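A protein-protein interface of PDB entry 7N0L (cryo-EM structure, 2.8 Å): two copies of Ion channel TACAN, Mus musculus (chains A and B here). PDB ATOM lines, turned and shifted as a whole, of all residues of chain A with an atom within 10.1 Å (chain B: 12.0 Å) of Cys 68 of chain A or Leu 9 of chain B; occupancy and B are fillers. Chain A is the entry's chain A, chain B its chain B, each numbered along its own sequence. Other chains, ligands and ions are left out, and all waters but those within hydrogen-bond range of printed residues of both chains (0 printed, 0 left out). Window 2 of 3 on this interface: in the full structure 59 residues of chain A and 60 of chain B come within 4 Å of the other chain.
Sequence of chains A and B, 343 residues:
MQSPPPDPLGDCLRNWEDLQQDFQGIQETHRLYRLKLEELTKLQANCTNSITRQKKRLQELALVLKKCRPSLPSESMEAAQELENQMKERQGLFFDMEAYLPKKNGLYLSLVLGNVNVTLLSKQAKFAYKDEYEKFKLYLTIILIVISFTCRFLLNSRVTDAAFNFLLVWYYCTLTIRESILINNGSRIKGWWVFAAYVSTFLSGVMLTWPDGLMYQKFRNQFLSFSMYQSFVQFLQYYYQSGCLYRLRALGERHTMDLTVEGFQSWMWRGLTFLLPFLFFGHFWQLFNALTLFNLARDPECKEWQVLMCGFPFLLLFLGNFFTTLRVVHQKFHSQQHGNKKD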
ATOM      1  N   LEU A  61       8.901  -3.422  -3.966  1.00  0.00           N
ATOM      2  CA  LEU A  61      10.160  -3.004  -4.572  1.00  0.00           C
ATOM      3  C   LEU A  61      10.276  -1.485  -4.603  1.00  0.00           C
ATOM      4  O   LEU A  61      11.372  -0.934  -4.444  1.00  0.00           O
ATOM      5  CB  LEU A  61      10.275  -3.590  -5.982  1.00  0.00           C
ATOM      6  CG  LEU A  61      11.519  -3.342  -6.848  1.00  0.00           C
ATOM      7  CD1 LEU A  61      11.372  -2.079  -7.694  1.00  0.00           C
ATOM      8  CD2 LEU A  61      12.794  -3.304  -6.013  1.00  0.00           C
ATOM      9  N   ALA A  62       9.153  -0.789  -4.795  1.00  0.00           N
ATOM     10  CA  ALA A  62       9.195   0.667  -4.888  1.00  0.00           C
ATOM     11  C   ALA A  62       9.539   1.301  -3.545  1.00  0.00           C
ATOM     12  O   ALA A  62      10.352   2.230  -3.483  1.00  0.00           O
ATOM     13  CB  ALA A  62       7.861   1.199  -5.409  1.00  0.00           C
ATOM     14  N   LEU A  63       8.932   0.814  -2.461  1.00  0.00           N
ATOM     15  CA  LEU A  63       9.212   1.380  -1.146  1.00  0.00           C
ATOM     16  C   LEU A  63      10.653   1.119  -0.729  1.00  0.00           C
ATOM     17  O   LEU A  63      11.288   1.974  -0.104  1.00  0.00           O
ATOM     18  CB  LEU A  63       8.235   0.818  -0.114  1.00  0.00           C
ATOM     19  CG  LEU A  63       6.757   0.873  -0.503  1.00  0.00           C
ATOM     20  CD1 LEU A  63       5.880   0.405   0.647  1.00  0.00           C
ATOM     21  CD2 LEU A  63       6.367   2.279  -0.942  1.00  0.00           C
ATOM     22  N   VAL A  64      11.185  -0.059  -1.067  1.00  0.00           N
ATOM     23  CA  VAL A  64      12.599  -0.336  -0.841  1.00  0.00           C
ATOM     24  C   VAL A  64      13.470   0.619  -1.644  1.00  0.00           C
ATOM     25  O   VAL A  64      14.604   0.910  -1.251  1.00  0.00           O
ATOM     26  CB  VAL A  64      12.901  -1.814  -1.177  1.00  0.00           C
ATOM     27  CG1 VAL A  64      14.399  -2.096  -1.156  1.00  0.00           C
ATOM     28  CG2 VAL A  64      12.172  -2.732  -0.207  1.00  0.00           C
ATOM     29  N   LEU A  65      12.953   1.146  -2.751  1.00  0.00           N
ATOM     30  CA  LEU A  65      13.663   2.156  -3.524  1.00  0.00           C
ATOM     31  C   LEU A  65      13.322   3.570  -3.074  1.00  0.00           C
ATOM     32  O   LEU A  65      14.180   4.458  -3.117  1.00  0.00           O
ATOM     33  CB  LEU A  65      13.348   1.997  -5.013  1.00  0.00           C
ATOM     34  CG  LEU A  65      14.093   2.927  -5.968  1.00  0.00           C
ATOM     35  CD1 LEU A  65      15.555   2.534  -6.065  1.00  0.00           C
ATOM     36  CD2 LEU A  65      13.441   2.914  -7.338  1.00  0.00           C
ATOM     37  N   LYS A  66      12.079   3.793  -2.637  1.00  0.00           N
ATOM     38  CA  LYS A  66      11.639   5.143  -2.304  1.00  0.00           C
ATOM     39  C   LYS A  66      12.408   5.722  -1.123  1.00  0.00           C
ATOM     40  O   LYS A  66      12.578   6.943  -1.037  1.00  0.00           O
ATOM     41  CB  LYS A  66      10.137   5.144  -2.011  1.00  0.00           C
ATOM     42  CG  LYS A  66       9.546   6.528  -1.813  1.00  0.00           C
ATOM     43  CD  LYS A  66       8.380   6.502  -0.842  1.00  0.00           C
ATOM     44  CE  LYS A  66       7.202   7.289  -1.389  1.00  0.00           C
ATOM     45  NZ  LYS A  66       7.652   8.414  -2.252  1.00  0.00           N
ATOM     46  N   LYS A  67      12.882   4.874  -0.208  1.00  0.00           N
ATOM     47  CA  LYS A  67      13.583   5.387   0.962  1.00  0.00           C
ATOM     48  C   LYS A  67      15.008   5.827   0.645  1.00  0.00           C
ATOM     49  O   LYS A  67      15.580   6.620   1.401  1.00  0.00           O
ATOM     50  CB  LYS A  67      13.574   4.345   2.090  1.00  0.00           C
ATOM     51  CG  LYS A  67      14.015   2.918   1.730  1.00  0.00           C
ATOM     52  CD  LYS A  67      15.525   2.784   1.544  1.00  0.00           C
ATOM     53  CE  LYS A  67      15.957   1.327   1.495  1.00  0.00           C
ATOM     54  NZ  LYS A  67      17.168   1.133   0.652  1.00  0.00           N
ATOM     55  N   CYS A  68      15.591   5.339  -0.449  1.00  0.00           N
ATOM     56  CA  CYS A  68      16.995   5.603  -0.737  1.00  0.00           C
ATOM     57  C   CYS A  68      17.206   6.838  -1.601  1.00  0.00           C
ATOM     58  O   CYS A  68      18.218   7.529  -1.435  1.00  0.00           O
ATOM     59  CB  CYS A  68      17.630   4.389  -1.421  1.00  0.00           C
ATOM     60  SG  CYS A  68      19.414   4.532  -1.695  1.00  0.00           S
ATOM     61  N   ARG A  69      16.282   7.127  -2.517  1.00  0.00           N
ATOM     62  CA  ARG A  69      16.448   8.282  -3.393  1.00  0.00           C
ATOM     63  C   ARG A  69      16.597   9.613  -2.653  1.00  0.00           C
ATOM     64  O   ARG A  69      17.324  10.479  -3.168  1.00  0.00           O
ATOM     65  CB  ARG A  69      15.276   8.347  -4.385  1.00  0.00           C
ATOM     66  CG  ARG A  69      15.562   7.669  -5.717  1.00  0.00           C
ATOM     67  CD  ARG A  69      14.487   7.983  -6.744  1.00  0.00           C
ATOM     68  NE  ARG A  69      13.165   7.559  -6.294  1.00  0.00           N
ATOM     69  CZ  ARG A  69      12.071   7.599  -7.049  1.00  0.00           C
ATOM     70  NH1 ARG A  69      12.140   8.045  -8.296  1.00  0.00           N
ATOM     71  NH2 ARG A  69      10.908   7.193  -6.558  1.00  0.00           N
ATOM     72  N   PRO A  70      15.963   9.852  -1.499  1.00  0.00           N
ATOM     73  CA  PRO A  70      16.300  11.077  -0.757  1.00  0.00           C
ATOM     74  C   PRO A  70      17.695  11.046  -0.161  1.00  0.00           C
ATOM     75  O   PRO A  70      18.358  12.089  -0.095  1.00  0.00           O
ATOM     76  CB  PRO A  70      15.216  11.137   0.329  1.00  0.00           C
ATOM     77  CG  PRO A  70      14.081  10.358  -0.233  1.00  0.00           C
ATOM     78  CD  PRO A  70      14.729   9.236  -0.980  1.00  0.00           C
ATOM     79  N   SER A  71      18.164   9.876   0.277  1.00  0.00           N
ATOM     80  CA  SER A  71      19.470   9.768   0.914  1.00  0.00           C
ATOM     81  C   SER A  71      20.593   9.463  -0.068  1.00  0.00           C
ATOM     82  O   SER A  71      21.753   9.759   0.241  1.00  0.00           O
ATOM     83  CB  SER A  71      19.444   8.688   2.001  1.00  0.00           C
ATOM     84  OG  SER A  71      20.017   7.479   1.536  1.00  0.00           O
ATOM     85  N   LEU A  72      20.272   8.895  -1.231  1.00  0.00           N
ATOM     86  CA  LEU A  72      21.237   8.539  -2.281  1.00  0.00           C
ATOM     87  C   LEU A  72      22.566   8.005  -1.747  1.00  0.00           C
ATOM     88  O   LEU A  72      23.617   8.212  -2.352  1.00  0.00           O
ATOM     89  CB  LEU A  72      21.498   9.742  -3.201  1.00  0.00           C
ATOM     90  CG  LEU A  72      21.947  11.085  -2.621  1.00  0.00           C
ATOM     91  CD1 LEU A  72      23.038  11.710  -3.475  1.00  0.00           C
ATOM     92  CD2 LEU A  72      20.764  12.028  -2.494  1.00  0.00           C
ATOM     93  N   SER A  76      24.157   9.898 -10.604  1.00  0.00           N
ATOM     94  CA  SER A  76      23.533   8.600 -10.833  1.00  0.00           C
ATOM     95  C   SER A  76      22.139   8.555 -10.219  1.00  0.00           C
ATOM     96  O   SER A  76      21.431   7.556 -10.344  1.00  0.00           O
ATOM     97  CB  SER A  76      24.398   7.477 -10.258  1.00  0.00           C
ATOM     98  OG  SER A  76      25.324   7.002 -11.218  1.00  0.00           O
ATOM     99  N   MET A  77      21.753   9.648  -9.556  1.00  0.00           N
ATOM    100  CA  MET A  77      20.457   9.711  -8.889  1.00  0.00           C
ATOM    101  C   MET A  77      19.296   9.503  -9.851  1.00  0.00           C
ATOM    102  O   MET A  77      18.209   9.108  -9.417  1.00  0.00           O
ATOM    103  CB  MET A  77      20.304  11.052  -8.172  1.00  0.00           C
ATOM    104  CG  MET A  77      21.416  11.342  -7.186  1.00  0.00           C
ATOM    105  SD  MET A  77      22.842  12.088  -7.998  1.00  0.00           S
ATOM    106  CE  MET A  77      24.173  11.519  -6.944  1.00  0.00           C
ATOM    107  N   GLU A  78      19.497   9.759 -11.143  1.00  0.00           N
ATOM    108  CA  GLU A  78      18.467   9.485 -12.135  1.00  0.00           C
ATOM    109  C   GLU A  78      18.526   8.063 -12.669  1.00  0.00           C
ATOM    110  O   GLU A  78      17.509   7.558 -13.156  1.00  0.00           O
ATOM    111  CB  GLU A  78      18.554  10.485 -13.295  1.00  0.00           C
ATOM    112  CG  GLU A  78      17.979  11.868 -12.979  1.00  0.00           C
ATOM    113  CD  GLU A  78      18.579  12.497 -11.737  1.00  0.00           C
ATOM    114  OE1 GLU A  78      17.935  12.432 -10.667  1.00  0.00           O
ATOM    115  OE2 GLU A  78      19.695  13.050 -11.828  1.00  0.00           O
ATOM    116  N   ALA A  79      19.687   7.406 -12.588  1.00  0.00           N
ATOM    117  CA  ALA A  79      19.736   5.976 -12.865  1.00  0.00           C
ATOM    118  C   ALA A  79      18.919   5.196 -11.846  1.00  0.00           C
ATOM    119  O   ALA A  79      18.421   4.106 -12.150  1.00  0.00           O
ATOM    120  CB  ALA A  79      21.185   5.489 -12.877  1.00  0.00           C
ATOM    121  N   ALA A  80      18.784   5.728 -10.631  1.00  0.00           N
ATOM    122  CA  ALA A  80      17.886   5.122  -9.656  1.00  0.00           C
ATOM    123  C   ALA A  80      16.430   5.435  -9.980  1.00  0.00           C
ATOM    124  O   ALA A  80      15.562   4.563  -9.858  1.00  0.00           O
ATOM    125  CB  ALA A  80      18.239   5.597  -8.248  1.00  0.00           C
ATOM    126  N   GLN A  81      16.141   6.671 -10.394  1.00  0.00           N
ATOM    127  CA  GLN A  81      14.767   7.046 -10.701  1.00  0.00           C
ATOM    128  C   GLN A  81      14.323   6.581 -12.081  1.00  0.00           C
ATOM    129  O   GLN A  81      13.144   6.737 -12.415  1.00  0.00           O
ATOM    130  CB  GLN A  81      14.577   8.561 -10.595  1.00  0.00           C
ATOM    131  CG  GLN A  81      15.025   9.337 -11.819  1.00  0.00           C
ATOM    132  CD  GLN A  81      14.062  10.443 -12.195  1.00  0.00           C
ATOM    133  OE1 GLN A  81      13.022  10.619 -11.561  1.00  0.00           O
ATOM    134  NE2 GLN A  81      14.407  11.200 -13.231  1.00  0.00           N
ATOM    135  N   GLU A  82      15.222   6.027 -12.892  1.00  0.00           N
ATOM    136  CA  GLU A  82      14.767   5.376 -14.111  1.00  0.00           C
ATOM    137  C   GLU A  82      14.147   4.019 -13.818  1.00  0.00           C
ATOM    138  O   GLU A  82      13.588   3.396 -14.726  1.00  0.00           O
ATOM    139  CB  GLU A  82      15.917   5.238 -15.117  1.00  0.00           C
ATOM    140  CG  GLU A  82      16.881   4.094 -14.860  1.00  0.00           C
ATOM    141  CD  GLU A  82      16.469   2.817 -15.573  1.00  0.00           C
ATOM    142  OE1 GLU A  82      16.257   1.793 -14.892  1.00  0.00           O
ATOM    143  OE2 GLU A  82      16.353   2.846 -16.816  1.00  0.00           O
ATOM    144  N   LEU A  83      14.244   3.546 -12.574  1.00  0.00           N
ATOM    145  CA  LEU A  83      13.421   2.425 -12.146  1.00  0.00           C
ATOM    146  C   LEU A  83      11.959   2.833 -12.026  1.00  0.00           C
ATOM    147  O   LEU A  83      11.070   1.982 -12.136  1.00  0.00           O
ATOM    148  CB  LEU A  83      13.933   1.869 -10.818  1.00  0.00           C
ATOM    149  CG  LEU A  83      14.813   0.621 -10.888  1.00  0.00           C
ATOM    150  CD1 LEU A  83      14.063  -0.525 -11.544  1.00  0.00           C
ATOM    151  CD2 LEU A  83      16.106   0.914 -11.631  1.00  0.00           C
ATOM    152  N   LEU B   9      20.020   0.804  -5.864  1.00  0.00           N
ATOM    153  CA  LEU B   9      21.385   0.299  -5.929  1.00  0.00           C
ATOM    154  C   LEU B   9      21.486  -0.904  -6.859  1.00  0.00           C
ATOM    155  O   LEU B   9      20.570  -1.180  -7.635  1.00  0.00           O
ATOM    156  CB  LEU B   9      21.886  -0.075  -4.532  1.00  0.00           C
ATOM    157  CG  LEU B   9      22.031   1.074  -3.533  1.00  0.00           C
ATOM    158  CD1 LEU B   9      20.871   1.079  -2.552  1.00  0.00           C
ATOM    159  CD2 LEU B   9      23.360   0.983  -2.796  1.00  0.00           C
ATOM    160  N   GLY B  10      22.610  -1.610  -6.780  1.00  0.00           N
ATOM    161  CA  GLY B  10      22.824  -2.789  -7.595  1.00  0.00           C
ATOM    162  C   GLY B  10      21.816  -3.885  -7.321  1.00  0.00           C
ATOM    163  O   GLY B  10      21.114  -4.334  -8.231  1.00  0.00           O
ATOM    164  N   ASP B  11      21.735  -4.326  -6.062  1.00  0.00           N
ATOM    165  CA  ASP B  11      20.779  -5.370  -5.712  1.00  0.00           C
ATOM    166  C   ASP B  11      19.342  -4.877  -5.824  1.00  0.00           C
ATOM    167  O   ASP B  11      18.427  -5.685  -6.019  1.00  0.00           O
ATOM    168  CB  ASP B  11      21.052  -5.892  -4.301  1.00  0.00           C
ATOM    169  CG  ASP B  11      20.741  -7.371  -4.160  1.00  0.00           C
ATOM    170  OD1 ASP B  11      19.771  -7.713  -3.452  1.00  0.00           O
ATOM    171  OD2 ASP B  11      21.467  -8.189  -4.761  1.00  0.00           O
ATOM    172  N   CYS B  12      19.126  -3.564  -5.695  1.00  0.00           N
ATOM    173  CA  CYS B  12      17.787  -3.013  -5.870  1.00  0.00           C
ATOM    174  C   CYS B  12      17.250  -3.283  -7.270  1.00  0.00           C
ATOM    175  O   CYS B  12      16.033  -3.383  -7.459  1.00  0.00           O
ATOM    176  CB  CYS B  12      17.793  -1.512  -5.583  1.00  0.00           C
ATOM    177  SG  CYS B  12      16.245  -0.872  -4.909  1.00  0.00           S
ATOM    178  N   LEU B  13      18.135  -3.393  -8.259  1.00  0.00           N
ATOM    179  CA  LEU B  13      17.735  -3.837  -9.586  1.00  0.00           C
ATOM    180  C   LEU B  13      17.860  -5.345  -9.756  1.00  0.00           C
ATOM    181  O   LEU B  13      17.192  -5.916 -10.626  1.00  0.00           O
ATOM    182  CB  LEU B  13      18.568  -3.120 -10.657  1.00  0.00           C
ATOM    183  CG  LEU B  13      18.238  -3.411 -12.124  1.00  0.00           C
ATOM    184  CD1 LEU B  13      17.877  -2.134 -12.870  1.00  0.00           C
ATOM    185  CD2 LEU B  13      19.397  -4.122 -12.803  1.00  0.00           C
ATOM    186  N   ARG B  14      18.687  -6.001  -8.938  1.00  0.00           N
ATOM    187  CA  ARG B  14      18.785  -7.456  -8.998  1.00  0.00           C
ATOM    188  C   ARG B  14      17.452  -8.108  -8.662  1.00  0.00           C
ATOM    189  O   ARG B  14      17.032  -9.060  -9.329  1.00  0.00           O
ATOM    190  CB  ARG B  14      19.881  -7.949  -8.054  1.00  0.00           C
ATOM    191  N   ASN B  15      16.770  -7.609  -7.631  1.00  0.00           N
ATOM    192  CA  ASN B  15      15.422  -8.072  -7.332  1.00  0.00           C
ATOM    193  C   ASN B  15      14.395  -7.524  -8.311  1.00  0.00           C
ATOM    194  O   ASN B  15      13.329  -8.127  -8.475  1.00  0.00           O
ATOM    195  CB  ASN B  15      15.030  -7.685  -5.904  1.00  0.00           C
ATOM    196  CG  ASN B  15      13.784  -8.406  -5.426  1.00  0.00           C
ATOM    197  OD1 ASN B  15      13.557  -9.569  -5.760  1.00  0.00           O
ATOM    198  ND2 ASN B  15      12.967  -7.716  -4.640  1.00  0.00           N
ATOM    199  N   TRP B  16      14.693  -6.398  -8.964  1.00  0.00           N
ATOM    200  CA  TRP B  16      13.799  -5.877  -9.991  1.00  0.00           C
ATOM    201  C   TRP B  16      13.754  -6.792 -11.205  1.00  0.00           C
ATOM    202  O   TRP B  16      12.726  -6.863 -11.888  1.00  0.00           O
ATOM    203  CB  TRP B  16      14.237  -4.472 -10.401  1.00  0.00           C
ATOM    204  CG  TRP B  16      13.664  -4.012 -11.704  1.00  0.00           C
ATOM    205  CD1 TRP B  16      14.328  -3.870 -12.885  1.00  0.00           C
ATOM    206  CD2 TRP B  16      12.309  -3.627 -11.957  1.00  0.00           C
ATOM    207  NE1 TRP B  16      13.469  -3.424 -13.861  1.00  0.00           N
ATOM    208  CE2 TRP B  16      12.223  -3.267 -13.315  1.00  0.00           C
ATOM    209  CE3 TRP B  16      11.159  -3.554 -11.167  1.00  0.00           C
ATOM    210  CZ2 TRP B  16      11.034  -2.841 -13.900  1.00  0.00           C
ATOM    211  CZ3 TRP B  16       9.982  -3.131 -11.748  1.00  0.00           C
ATOM    212  CH2 TRP B  16       9.927  -2.780 -13.101  1.00  0.00           C
ATOM    213  N   GLU B  17      14.845  -7.503 -11.483  1.00  0.00           N
ATOM    214  CA  GLU B  17      14.895  -8.397 -12.632  1.00  0.00           C
ATOM    215  C   GLU B  17      14.457  -9.814 -12.296  1.00  0.00           C
ATOM    216  O   GLU B  17      13.921 -10.509 -13.166  1.00  0.00           O
ATOM    217  CB  GLU B  17      16.307  -8.414 -13.223  1.00  0.00           C
ATOM    218  CG  GLU B  17      16.770  -7.050 -13.689  1.00  0.00           C
ATOM    219  CD  GLU B  17      16.086  -6.622 -14.970  1.00  0.00           C
ATOM    220  OE1 GLU B  17      15.816  -5.413 -15.127  1.00  0.00           O
ATOM    221  OE2 GLU B  17      15.818  -7.496 -15.818  1.00  0.00           O
ATOM    222  N   ASP B  18      14.674 -10.260 -11.058  1.00  0.00           N
ATOM    223  CA  ASP B  18      14.157 -11.556 -10.638  1.00  0.00           C
ATOM    224  C   ASP B  18      12.635 -11.572 -10.574  1.00  0.00           C
ATOM    225  O   ASP B  18      12.042 -12.653 -10.493  1.00  0.00           O
ATOM    226  CB  ASP B  18      14.742 -11.944  -9.279  1.00  0.00           C
ATOM    227  CG  ASP B  18      15.028 -13.429  -9.172  1.00  0.00           C
ATOM    228  OD1 ASP B  18      14.072 -14.227  -9.256  1.00  0.00           O
ATOM    229  OD2 ASP B  18      16.211 -13.797  -9.007  1.00  0.00           O
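Of the 20 printed residues of chain A, 4 touch a printed residue of chain B.
Hydrophobic or aromatic side chains of chain A that line the printed part of chain B: Leu 61, Leu 65 and Leu 83.
Hydrophobic or aromatic side chains of chain B within 4 Å of the printed part of chain A: Leu 9, Leu 13 and Trp 16.
Among the printed residues, no Asp or Glu carboxylate lies within 4 Å of a Lys or Arg side-chain nitrogen of the other chain.
OE1 of Glu 17 of chain B lies close to NE1 of Trp 16 of chain B, at 3.3 Å.
OG of Ser 71 of chain A sits close to O of Cys 68 of chain A, at 3.5 Å.
No position is printed for both chains.
Cys 12 of chain B touches Leu 61 of chain A (O to CD2, 3.5 Å).
Leu 61 of chain A touches Trp 16 of chain B (CD1 to CE3, 3.8 Å).
CD1 of Leu 65 of chain A touches SG of Cys 12 of chain B, at 3.7 Å.
Leu 9 of chain B touches Cys 68 of chain A (CD1 to SG, 3.8 Å).
CD2 of Leu 83 of chain A touches CD1 of Leu 13 of chain B, 3.7 Å away.
CD1 of Leu 83 of chain A touches CG of Trp 16 of chain B, at 3.5 Å.
Printed residues of chain B within 4 Å of Leu 61 of chain A: Cys 12 (3.5 Å) and Trp 16 (3.8 Å).
Leu 63 of chain A touches none of the printed residues of chain B.
Of chain B, only Cys 12 (3.7 Å) comes within 4 Å of Leu 65 of chain A.
Lys 66 of chain A touches none of the printed residues of chain B.
Cys 68 of chain A touches just one residue of chain B: Leu 9 (3.8 Å).
No residue of chain B comes within 4 Å of Pro 70 of chain A.
No residue of chain B comes within 4 Å of Ser 71 of chain A.
Of the printed residues of chain B, Leu 83 of chain A touches Leu 13 and Trp 16.
Leu 9 of chain B touches one residue of chain A.
No residue of chain A comes within 4 Å of Gly 10 of chain B.
Of chain A, only Leu 61 (3.5 Å) and Leu 65 (3.7 Å) come within 4 Å of Cys 12 of chain B.
Printed residues of chain A within 4 Å of Leu 13 of chain B: Leu 83.
The nearest printed residue of chain B that does not touch Leu 83 of chain A is Cys 12 of chain B (5.4 Å).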
